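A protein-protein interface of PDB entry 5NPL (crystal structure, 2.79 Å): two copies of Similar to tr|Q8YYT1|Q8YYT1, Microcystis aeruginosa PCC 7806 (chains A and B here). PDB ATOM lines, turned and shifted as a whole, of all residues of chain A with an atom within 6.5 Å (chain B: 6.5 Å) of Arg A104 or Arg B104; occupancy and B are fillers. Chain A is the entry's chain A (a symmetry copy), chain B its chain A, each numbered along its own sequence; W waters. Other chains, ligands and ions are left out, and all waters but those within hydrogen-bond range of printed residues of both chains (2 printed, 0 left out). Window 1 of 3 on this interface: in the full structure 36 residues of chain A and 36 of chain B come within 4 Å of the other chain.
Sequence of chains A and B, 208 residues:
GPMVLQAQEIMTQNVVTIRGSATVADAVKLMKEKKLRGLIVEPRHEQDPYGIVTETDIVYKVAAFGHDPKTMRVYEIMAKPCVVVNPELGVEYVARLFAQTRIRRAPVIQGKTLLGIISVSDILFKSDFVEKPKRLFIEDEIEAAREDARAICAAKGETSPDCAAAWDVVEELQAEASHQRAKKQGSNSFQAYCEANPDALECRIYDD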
ATOM      1  N   GLU A  55      10.622 -32.611  12.226  1.00  0.00           N
ATOM      2  CA  GLU A  55      10.493 -32.604  13.681  1.00  0.00           C
ATOM      3  C   GLU A  55      10.049 -31.243  14.242  1.00  0.00           C
ATOM      4  O   GLU A  55       9.230 -31.179  15.146  1.00  0.00           O
ATOM      5  CB  GLU A  55      11.818 -33.015  14.335  1.00  0.00           C
ATOM      6  CG  GLU A  55      12.990 -32.076  14.065  1.00  0.00           C
ATOM      7  CD  GLU A  55      14.307 -32.589  14.622  1.00  0.00           C
ATOM      8  OE1 GLU A  55      14.331 -33.696  15.189  1.00  0.00           O
ATOM      9  OE2 GLU A  55      15.323 -31.843  14.530  1.00  0.00           O
ATOM     10  N   THR A  56      10.565 -30.155  13.681  1.00  0.00           N
ATOM     11  CA  THR A  56      10.206 -28.815  14.123  1.00  0.00           C
ATOM     12  C   THR A  56       8.771 -28.424  13.809  1.00  0.00           C
ATOM     13  O   THR A  56       8.110 -27.826  14.638  1.00  0.00           O
ATOM     14  CB  THR A  56      11.175 -27.800  13.533  1.00  0.00           C
ATOM     15  OG1 THR A  56      12.489 -28.098  14.018  1.00  0.00           O
ATOM     16  CG2 THR A  56      10.820 -26.382  13.920  1.00  0.00           C
ATOM     17  N   TYR A  60       6.725 -27.372  17.005  1.00  0.00           N
ATOM     18  CA  TYR A  60       6.232 -25.987  17.010  1.00  0.00           C
ATOM     19  C   TYR A  60       4.729 -25.887  16.748  1.00  0.00           C
ATOM     20  O   TYR A  60       4.057 -25.089  17.369  1.00  0.00           O
ATOM     21  CB  TYR A  60       6.969 -25.141  15.976  1.00  0.00           C
ATOM     22  CG  TYR A  60       8.412 -24.741  16.285  1.00  0.00           C
ATOM     23  CD1 TYR A  60       9.164 -25.312  17.339  1.00  0.00           C
ATOM     24  CD2 TYR A  60       9.037 -23.814  15.495  1.00  0.00           C
ATOM     25  CE1 TYR A  60      10.476 -24.942  17.578  1.00  0.00           C
ATOM     26  CE2 TYR A  60      10.342 -23.426  15.726  1.00  0.00           C
ATOM     27  CZ  TYR A  60      11.063 -23.989  16.770  1.00  0.00           C
ATOM     28  OH  TYR A  60      12.345 -23.548  16.952  1.00  0.00           O
ATOM     29  N   PHE A  98      20.461 -23.185   2.575  1.00  0.00           N
ATOM     30  CA  PHE A  98      19.889 -23.391   3.892  1.00  0.00           C
ATOM     31  C   PHE A  98      19.911 -22.102   4.731  1.00  0.00           C
ATOM     32  O   PHE A  98      18.919 -21.760   5.343  1.00  0.00           O
ATOM     33  CB  PHE A  98      20.594 -24.557   4.604  1.00  0.00           C
ATOM     34  CG  PHE A  98      20.178 -25.933   4.128  1.00  0.00           C
ATOM     35  CD1 PHE A  98      19.351 -26.140   3.008  1.00  0.00           C
ATOM     36  CD2 PHE A  98      20.644 -27.058   4.794  1.00  0.00           C
ATOM     37  CE1 PHE A  98      19.002 -27.422   2.587  1.00  0.00           C
ATOM     38  CE2 PHE A  98      20.274 -28.326   4.394  1.00  0.00           C
ATOM     39  CZ  PHE A  98      19.441 -28.493   3.290  1.00  0.00           C
ATOM     40  N   ARG A 102      16.521 -20.287   5.686  1.00  0.00           N
ATOM     41  CA  ARG A 102      16.310 -20.606   7.106  1.00  0.00           C
ATOM     42  C   ARG A 102      15.730 -22.002   7.351  1.00  0.00           C
ATOM     43  O   ARG A 102      14.985 -22.184   8.274  1.00  0.00           O
ATOM     44  CB  ARG A 102      15.512 -19.499   7.813  1.00  0.00           C
ATOM     45  CG  ARG A 102      16.204 -18.135   7.728  1.00  0.00           C
ATOM     46  CD  ARG A 102      16.036 -17.191   8.946  1.00  0.00           C
ATOM     47  NE  ARG A 102      16.829 -17.541  10.160  1.00  0.00           N
ATOM     48  CZ  ARG A 102      18.179 -17.540  10.277  1.00  0.00           C
ATOM     49  NH1 ARG A 102      18.994 -17.269   9.233  1.00  0.00           N
ATOM     50  NH2 ARG A 102      18.732 -17.856  11.454  1.00  0.00           N
ATOM     51  N   ILE A 103      16.137 -22.979   6.539  1.00  0.00           N
ATOM     52  CA  ILE A 103      15.747 -24.367   6.691  1.00  0.00           C
ATOM     53  C   ILE A 103      16.965 -25.168   7.091  1.00  0.00           C
ATOM     54  O   ILE A 103      18.097 -24.738   6.890  1.00  0.00           O
ATOM     55  CB  ILE A 103      15.125 -24.996   5.397  1.00  0.00           C
ATOM     56  CG1 ILE A 103      16.189 -25.193   4.306  1.00  0.00           C
ATOM     57  CG2 ILE A 103      13.943 -24.184   4.892  1.00  0.00           C
ATOM     58  CD1 ILE A 103      15.655 -25.571   2.931  1.00  0.00           C
ATOM     59  N   ARG A 104      16.716 -26.355   7.635  1.00  0.00           N
ATOM     60  CA  ARG A 104      17.782 -27.238   8.087  1.00  0.00           C
ATOM     61  C   ARG A 104      17.826 -28.557   7.374  1.00  0.00           C
ATOM     62  O   ARG A 104      18.713 -29.353   7.670  1.00  0.00           O
ATOM     63  CB  ARG A 104      17.655 -27.445   9.595  1.00  0.00           C
ATOM     64  CG  ARG A 104      17.880 -26.154  10.337  1.00  0.00           C
ATOM     65  CD  ARG A 104      16.802 -25.872  11.368  1.00  0.00           C
ATOM     66  NE  ARG A 104      17.291 -24.835  12.298  1.00  0.00           N
ATOM     67  CZ  ARG A 104      17.273 -23.513  12.094  1.00  0.00           C
ATOM     68  NH1 ARG A 104      16.826 -22.979  10.955  1.00  0.00           N
ATOM     69  NH2 ARG A 104      17.730 -22.727  13.053  1.00  0.00           N
ATOM     70  N   ARG A 105      16.898 -28.773   6.439  1.00  0.00           N
ATOM     71  CA  ARG A 105      16.821 -30.034   5.703  1.00  0.00           C
ATOM     72  C   ARG A 105      15.904 -29.872   4.488  1.00  0.00           C
ATOM     73  O   ARG A 105      14.990 -29.045   4.479  1.00  0.00           O
ATOM     74  CB  ARG A 105      16.395 -31.215   6.580  1.00  0.00           C
ATOM     75  CG  ARG A 105      14.896 -31.262   6.914  1.00  0.00           C
ATOM     76  CD  ARG A 105      14.490 -31.965   8.226  1.00  0.00           C
ATOM     77  NE  ARG A 105      15.595 -32.678   8.864  1.00  0.00           N
ATOM     78  CZ  ARG A 105      16.260 -32.298   9.969  1.00  0.00           C
ATOM     79  NH1 ARG A 105      15.931 -31.184  10.659  1.00  0.00           N
ATOM     80  NH2 ARG A 105      17.300 -33.042  10.360  1.00  0.00           N
ATOM     81  N   ALA A 106      16.200 -30.650   3.446  1.00  0.00           N
ATOM     82  CA  ALA A 106      15.500 -30.588   2.185  1.00  0.00           C
ATOM     83  C   ALA A 106      15.654 -31.902   1.475  1.00  0.00           C
ATOM     84  O   ALA A 106      16.672 -32.581   1.655  1.00  0.00           O
ATOM     85  CB  ALA A 106      16.098 -29.503   1.349  1.00  0.00           C
ATOM     86  N   ILE A 118      18.946 -34.281   2.731  1.00  0.00           N
ATOM     87  CA  ILE A 118      20.201 -33.632   3.124  1.00  0.00           C
ATOM     88  C   ILE A 118      19.863 -32.587   4.174  1.00  0.00           C
ATOM     89  O   ILE A 118      18.879 -31.843   4.041  1.00  0.00           O
ATOM     90  CB  ILE A 118      20.968 -32.991   1.926  1.00  0.00           C
ATOM     91  CG1 ILE A 118      22.347 -32.527   2.373  1.00  0.00           C
ATOM     92  CG2 ILE A 118      20.220 -31.819   1.260  1.00  0.00           C
ATOM     93  CD1 ILE A 118      23.318 -32.344   1.232  1.00  0.00           C
ATOM     94  N   SER A 119      20.671 -32.562   5.216  1.00  0.00           N
ATOM     95  CA  SER A 119      20.429 -31.711   6.360  1.00  0.00           C
ATOM     96  C   SER A 119      21.703 -31.018   6.819  1.00  0.00           C
ATOM     97  O   SER A 119      22.803 -31.376   6.432  1.00  0.00           O
ATOM     98  CB  SER A 119      19.887 -32.555   7.508  1.00  0.00           C
ATOM     99  OG  SER A 119      20.870 -33.498   7.922  1.00  0.00           O
ATOM    100  N   VAL A 120      21.524 -30.032   7.682  1.00  0.00           N
ATOM    101  CA  VAL A 120      22.657 -29.393   8.388  1.00  0.00           C
ATOM    102  C   VAL A 120      23.571 -30.420   9.104  1.00  0.00           C
ATOM    103  O   VAL A 120      24.775 -30.274   9.043  1.00  0.00           O
ATOM    104  CB  VAL A 120      22.221 -28.246   9.341  1.00  0.00           C
ATOM    105  CG1 VAL A 120      21.538 -27.135   8.581  1.00  0.00           C
ATOM    106  CG2 VAL A 120      21.261 -28.731  10.397  1.00  0.00           C
ATOM    107  N   SER A 121      23.014 -31.456   9.730  1.00  0.00           N
ATOM    108  CA  SER A 121      23.827 -32.523  10.354  1.00  0.00           C
ATOM    109  C   SER A 121      24.696 -33.223   9.335  1.00  0.00           C
ATOM    110  O   SER A 121      25.881 -33.439   9.561  1.00  0.00           O
ATOM    111  CB  SER A 121      22.958 -33.573  11.039  1.00  0.00           C
ATOM    112  OG  SER A 121      21.970 -32.971  11.854  1.00  0.00           O
ATOM    113  N   GLU B  55      24.992 -27.210  15.445  1.00  0.00           N
ATOM    114  CA  GLU B  55      25.227 -27.528  14.038  1.00  0.00           C
ATOM    115  C   GLU B  55      24.820 -26.391  13.086  1.00  0.00           C
ATOM    116  O   GLU B  55      25.519 -26.103  12.126  1.00  0.00           O
ATOM    117  CB  GLU B  55      24.478 -28.809  13.650  1.00  0.00           C
ATOM    118  CG  GLU B  55      22.959 -28.727  13.760  1.00  0.00           C
ATOM    119  CD  GLU B  55      22.269 -30.054  13.491  1.00  0.00           C
ATOM    120  OE1 GLU B  55      22.964 -31.057  13.255  1.00  0.00           O
ATOM    121  OE2 GLU B  55      21.005 -30.073  13.469  1.00  0.00           O
ATOM    122  N   THR B  56      23.707 -25.726  13.372  1.00  0.00           N
ATOM    123  CA  THR B  56      23.234 -24.623  12.546  1.00  0.00           C
ATOM    124  C   THR B  56      24.113 -23.386  12.605  1.00  0.00           C
ATOM    125  O   THR B  56      24.360 -22.768  11.585  1.00  0.00           O
ATOM    126  CB  THR B  56      21.800 -24.275  12.923  1.00  0.00           C
ATOM    127  OG1 THR B  56      20.977 -25.418  12.664  1.00  0.00           O
ATOM    128  CG2 THR B  56      21.272 -23.102  12.129  1.00  0.00           C
ATOM    129  N   TYR B  60      25.414 -22.250   9.066  1.00  0.00           N
ATOM    130  CA  TYR B  60      24.979 -20.913   8.634  1.00  0.00           C
ATOM    131  C   TYR B  60      26.093 -19.868   8.716  1.00  0.00           C
ATOM    132  O   TYR B  60      26.209 -19.036   7.839  1.00  0.00           O
ATOM    133  CB  TYR B  60      23.791 -20.431   9.460  1.00  0.00           C
ATOM    134  CG  TYR B  60      22.431 -21.078   9.189  1.00  0.00           C
ATOM    135  CD1 TYR B  60      22.272 -22.247   8.408  1.00  0.00           C
ATOM    136  CD2 TYR B  60      21.305 -20.535   9.749  1.00  0.00           C
ATOM    137  CE1 TYR B  60      21.028 -22.818   8.200  1.00  0.00           C
ATOM    138  CE2 TYR B  60      20.056 -21.086   9.543  1.00  0.00           C
ATOM    139  CZ  TYR B  60      19.916 -22.229   8.766  1.00  0.00           C
ATOM    140  OH  TYR B  60      18.649 -22.711   8.591  1.00  0.00           O
ATOM    141  N   PHE B  98      10.620 -23.333  23.009  1.00  0.00           N
ATOM    142  CA  PHE B  98      11.323 -23.508  21.751  1.00  0.00           C
ATOM    143  C   PHE B  98      10.613 -22.781  20.596  1.00  0.00           C
ATOM    144  O   PHE B  98      11.256 -22.099  19.823  1.00  0.00           O
ATOM    145  CB  PHE B  98      11.524 -25.004  21.457  1.00  0.00           C
ATOM    146  CG  PHE B  98      12.633 -25.661  22.252  1.00  0.00           C
ATOM    147  CD1 PHE B  98      13.310 -25.014  23.303  1.00  0.00           C
ATOM    148  CD2 PHE B  98      12.996 -26.969  21.968  1.00  0.00           C
ATOM    149  CE1 PHE B  98      14.314 -25.656  24.025  1.00  0.00           C
ATOM    150  CE2 PHE B  98      14.011 -27.594  22.664  1.00  0.00           C
ATOM    151  CZ  PHE B  98      14.671 -26.918  23.689  1.00  0.00           C
ATOM    152  N   ARG B 102      12.318 -19.651  18.865  1.00  0.00           N
ATOM    153  CA  ARG B 102      12.810 -20.156  17.575  1.00  0.00           C
ATOM    154  C   ARG B 102      14.129 -20.928  17.670  1.00  0.00           C
ATOM    155  O   ARG B 102      14.917 -20.875  16.767  1.00  0.00           O
ATOM    156  CB  ARG B 102      12.851 -19.040  16.519  1.00  0.00           C
ATOM    157  CG  ARG B 102      11.476 -18.402  16.290  1.00  0.00           C
ATOM    158  CD  ARG B 102      11.161 -17.926  14.849  1.00  0.00           C
ATOM    159  NE  ARG B 102      10.852 -18.997  13.859  1.00  0.00           N
ATOM    160  CZ  ARG B 102       9.788 -19.835  13.873  1.00  0.00           C
ATOM    161  NH1 ARG B 102       8.878 -19.831  14.874  1.00  0.00           N
ATOM    162  NH2 ARG B 102       9.646 -20.727  12.886  1.00  0.00           N
ATOM    163  N   ILE B 103      14.313 -21.685  18.754  1.00  0.00           N
ATOM    164  CA  ILE B 103      15.467 -22.538  18.954  1.00  0.00           C
ATOM    165  C   ILE B 103      15.013 -23.980  18.905  1.00  0.00           C
ATOM    166  O   ILE B 103      13.836 -24.277  19.086  1.00  0.00           O
ATOM    167  CB  ILE B 103      16.216 -22.284  20.307  1.00  0.00           C
ATOM    168  CG1 ILE B 103      15.384 -22.769  21.505  1.00  0.00           C
ATOM    169  CG2 ILE B 103      16.626 -20.828  20.455  1.00  0.00           C
ATOM    170  CD1 ILE B 103      15.907 -22.357  22.874  1.00  0.00           C
ATOM    171  N   ARG B 104      15.971 -24.875  18.688  1.00  0.00           N
ATOM    172  CA  ARG B 104      15.692 -26.302  18.598  1.00  0.00           C
ATOM    173  C   ARG B 104      16.377 -27.125  19.648  1.00  0.00           C
ATOM    174  O   ARG B 104      16.175 -28.336  19.666  1.00  0.00           O
ATOM    175  CB  ARG B 104      16.057 -26.796  17.201  1.00  0.00           C
ATOM    176  CG  ARG B 104      15.177 -26.162  16.156  1.00  0.00           C
ATOM    177  CD  ARG B 104      15.964 -25.589  14.992  1.00  0.00           C
ATOM    178  NE  ARG B 104      15.042 -25.355  13.862  1.00  0.00           N
ATOM    179  CZ  ARG B 104      14.247 -24.293  13.692  1.00  0.00           C
ATOM    180  NH1 ARG B 104      14.177 -23.311  14.593  1.00  0.00           N
ATOM    181  NH2 ARG B 104      13.504 -24.238  12.601  1.00  0.00           N
ATOM    182  N   ARG B 105      17.158 -26.477  20.514  1.00  0.00           N
ATOM    183  CA  ARG B 105      17.905 -27.178  21.559  1.00  0.00           C
ATOM    184  C   ARG B 105      18.423 -26.174  22.590  1.00  0.00           C
ATOM    185  O   ARG B 105      18.657 -25.002  22.285  1.00  0.00           O
ATOM    186  CB  ARG B 105      19.031 -28.054  21.004  1.00  0.00           C
ATOM    187  CG  ARG B 105      20.285 -27.285  20.557  1.00  0.00           C
ATOM    188  CD  ARG B 105      21.151 -27.934  19.457  1.00  0.00           C
ATOM    189  NE  ARG B 105      20.756 -29.306  19.146  1.00  0.00           N
ATOM    190  CZ  ARG B 105      20.103 -29.721  18.047  1.00  0.00           C
ATOM    191  NH1 ARG B 105      19.765 -28.876  17.049  1.00  0.00           N
ATOM    192  NH2 ARG B 105      19.756 -31.011  17.975  1.00  0.00           N
ATOM    193  N   ALA B 106      18.556 -26.650  23.830  1.00  0.00           N
ATOM    194  CA  ALA B 106      18.957 -25.838  24.953  1.00  0.00           C
ATOM    195  C   ALA B 106      19.553 -26.724  26.009  1.00  0.00           C
ATOM    196  O   ALA B 106      19.164 -27.894  26.118  1.00  0.00           O
ATOM    197  CB  ALA B 106      17.754 -25.148  25.510  1.00  0.00           C
ATOM    198  N   ILE B 118      18.471 -30.829  25.769  1.00  0.00           N
ATOM    199  CA  ILE B 118      17.120 -31.198  25.332  1.00  0.00           C
ATOM    200  C   ILE B 118      16.863 -30.498  24.009  1.00  0.00           C
ATOM    201  O   ILE B 118      17.190 -29.313  23.839  1.00  0.00           O
ATOM    202  CB  ILE B 118      16.014 -30.843  26.374  1.00  0.00           C
ATOM    203  CG1 ILE B 118      14.681 -31.441  25.948  1.00  0.00           C
ATOM    204  CG2 ILE B 118      15.847 -29.331  26.619  1.00  0.00           C
ATOM    205  CD1 ILE B 118      13.691 -31.570  27.080  1.00  0.00           C
ATOM    206  N   SER B 119      16.302 -31.249  23.080  1.00  0.00           N
ATOM    207  CA  SER B 119      16.094 -30.777  21.729  1.00  0.00           C
ATOM    208  C   SER B 119      14.708 -31.143  21.219  1.00  0.00           C
ATOM    209  O   SER B 119      14.010 -31.963  21.791  1.00  0.00           O
ATOM    210  CB  SER B 119      17.137 -31.404  20.812  1.00  0.00           C
ATOM    211  OG  SER B 119      16.956 -32.817  20.768  1.00  0.00           O
ATOM    212  N   VAL B 120      14.342 -30.530  20.105  1.00  0.00           N
ATOM    213  CA  VAL B 120      13.125 -30.920  19.360  1.00  0.00           C
ATOM    214  C   VAL B 120      13.077 -32.436  19.043  1.00  0.00           C
ATOM    215  O   VAL B 120      12.025 -33.029  19.174  1.00  0.00           O
ATOM    216  CB  VAL B 120      12.876 -30.058  18.092  1.00  0.00           C
ATOM    217  CG1 VAL B 120      12.685 -28.603  18.449  1.00  0.00           C
ATOM    218  CG2 VAL B 120      14.030 -30.140  17.124  1.00  0.00           C
ATOM    219  N   SER B 121      14.198 -33.056  18.677  1.00  0.00           N
ATOM    220  CA  SER B 121      14.247 -34.517  18.449  1.00  0.00           C
ATOM    221  C   SER B 121      13.878 -35.283  19.698  1.00  0.00           C
ATOM    222  O   SER B 121      13.084 -36.216  19.653  1.00  0.00           O
ATOM    223  CB  SER B 121      15.631 -34.978  18.001  1.00  0.00           C
ATOM    224  OG  SER B 121      16.134 -34.158  16.963  1.00  0.00           O
HETATM  225  O   HOH W   1      19.606 -31.753  11.853  1.00  0.00           O
HETATM  226  O   HOH W   2      17.289 -31.828  16.407  1.00  0.00           O
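Of the 13 printed residues of chain A, 9 touch a printed residue of chain B. Hydrophobic or aromatic side chains of chain A within 4 Å of the printed part of chain B: Tyr A60 and Val A120. Printed residues of chain B that touch a printed residue of chain A: Glu B55, Thr B56, Tyr B60, Phe B98, Arg B102, Ile B103, Arg B104, Val B120 and Ser B121. Along chain B the printed residues that touch a printed residue of chain A span positions 55 to 121. Among the printed residues, 15 pairs touch across the chains. Among the printed residues, no Asp or Glu carboxylate lies within 4 Å of a Lys or Arg side-chain nitrogen of the other chain.
The backbone carbonyl oxygen (O) of Ile B103 sits at hydrogen-bond distance from the side-chain hydroxyl (OH) of Tyr A60 (2.7 Å). O of Phe B98 lies within hydrogen-bond range of OH of Tyr A60, at 3.4 Å. NE of Arg B104 lies close to NE of Arg A104 (2.8 Å). The side-chain hydroxyl of Tyr B60 sits at hydrogen-bond distance from the backbone carbonyl oxygen of Phe A98 (3.4 Å). OH of Tyr B60 is in hydrogen-bond range of NH1 of Arg A104. OE1 of Glu A55 sits at hydrogen-bond distance from OG of Ser B121, at 2.6 Å. The guanidinium group (NH1) of Arg B104 lies within hydrogen-bond range of the side-chain hydroxyl (OH) of Tyr A60 (3.0 Å). The side-chain carboxylate (OE1) of Glu B55 sits at hydrogen-bond distance from the side-chain hydroxyl (OG) of Ser A121, at 2.6 Å. The side-chain hydroxyl (OH) of Tyr B60 sits at hydrogen-bond distance from the backbone carbonyl oxygen (O) of Ile A103 (2.7 Å).
Of the printed residues of chain B, Ile A103 touches Tyr B60. Of chain B, only Thr B56 (3.7 Å), Tyr B60 (3.0 Å) and Arg B104 (2.8 Å) come within 4 Å of Arg A104. Printed residues of chain A within 4 Å of Arg B102: Tyr A60. The nearest residue of chain A that does not touch Arg B104 is Arg A102 (5.0 Å).
Water W2 lies within hydrogen-bond range of OG of Ser B121, OE2 of Glu A55 and NH2 of Arg B105. Water W1 lies within hydrogen-bond range of the side-chain hydroxyl (OG) of Ser A121 (2.7 Å), the side-chain carboxylate (OE2) of Glu B55 (2.7 Å) and the guanidinium group (NH2) of Arg A105 (3.0 Å).
O of Arg A104 lies within hydrogen-bond range of N of Val A120 (2.9 Å). The backbone carbonyl oxygen (O) of Arg A102 is in hydrogen-bond range of the guanidinium group (NH1) of Arg A104. The backbone carbonyl oxygen (O) of Phe B98 sits at hydrogen-bond distance from the backbone NH (N) of Ile B103. The side-chain carboxylate (OE2) of Glu A55 is in salt-bridge range of the guanidinium group (NH1) of Arg A105, 3.97 Å away. O of Phe A98 sits at hydrogen-bond distance from N of Ile A103 (3.3 Å). The backbone NH of Ser A121 sits close to the side-chain hydroxyl of Ser A119 (3.5 Å).
Glu A55 touches Val B120, and with the chains exchanged Val A120 touches Glu B55. Tyr A60 touches Phe B98, and with the chains exchanged Phe A98 touches Tyr B60. Tyr A60 touches Arg B102, and with the chains exchanged Arg A102 touches Tyr B60. Tyr A60 touches Ile B103, and with the chains exchanged Ile A103 touches Tyr B60. Positions printed for both chains: 55, 56, 60, 98, 102, 103, 104, 105, 106, 118, 119, 120 and 121.
CG2 of Val B120 touches OE2 of Glu A55, 3.4 Å away. Thr A56 touches Arg B104 (CG2 to NH2, 3.7 Å). Arg B102 touches Tyr A60 (C to OH, 3.3 Å). C of Arg A102 touches OH of Tyr B60, 3.2 Å away. Thr B56 touches Arg A104 (CG2 to NH2, 3.7 Å). CG2 of Val A120 touches OE2 of Glu B55 (3.4 Å).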
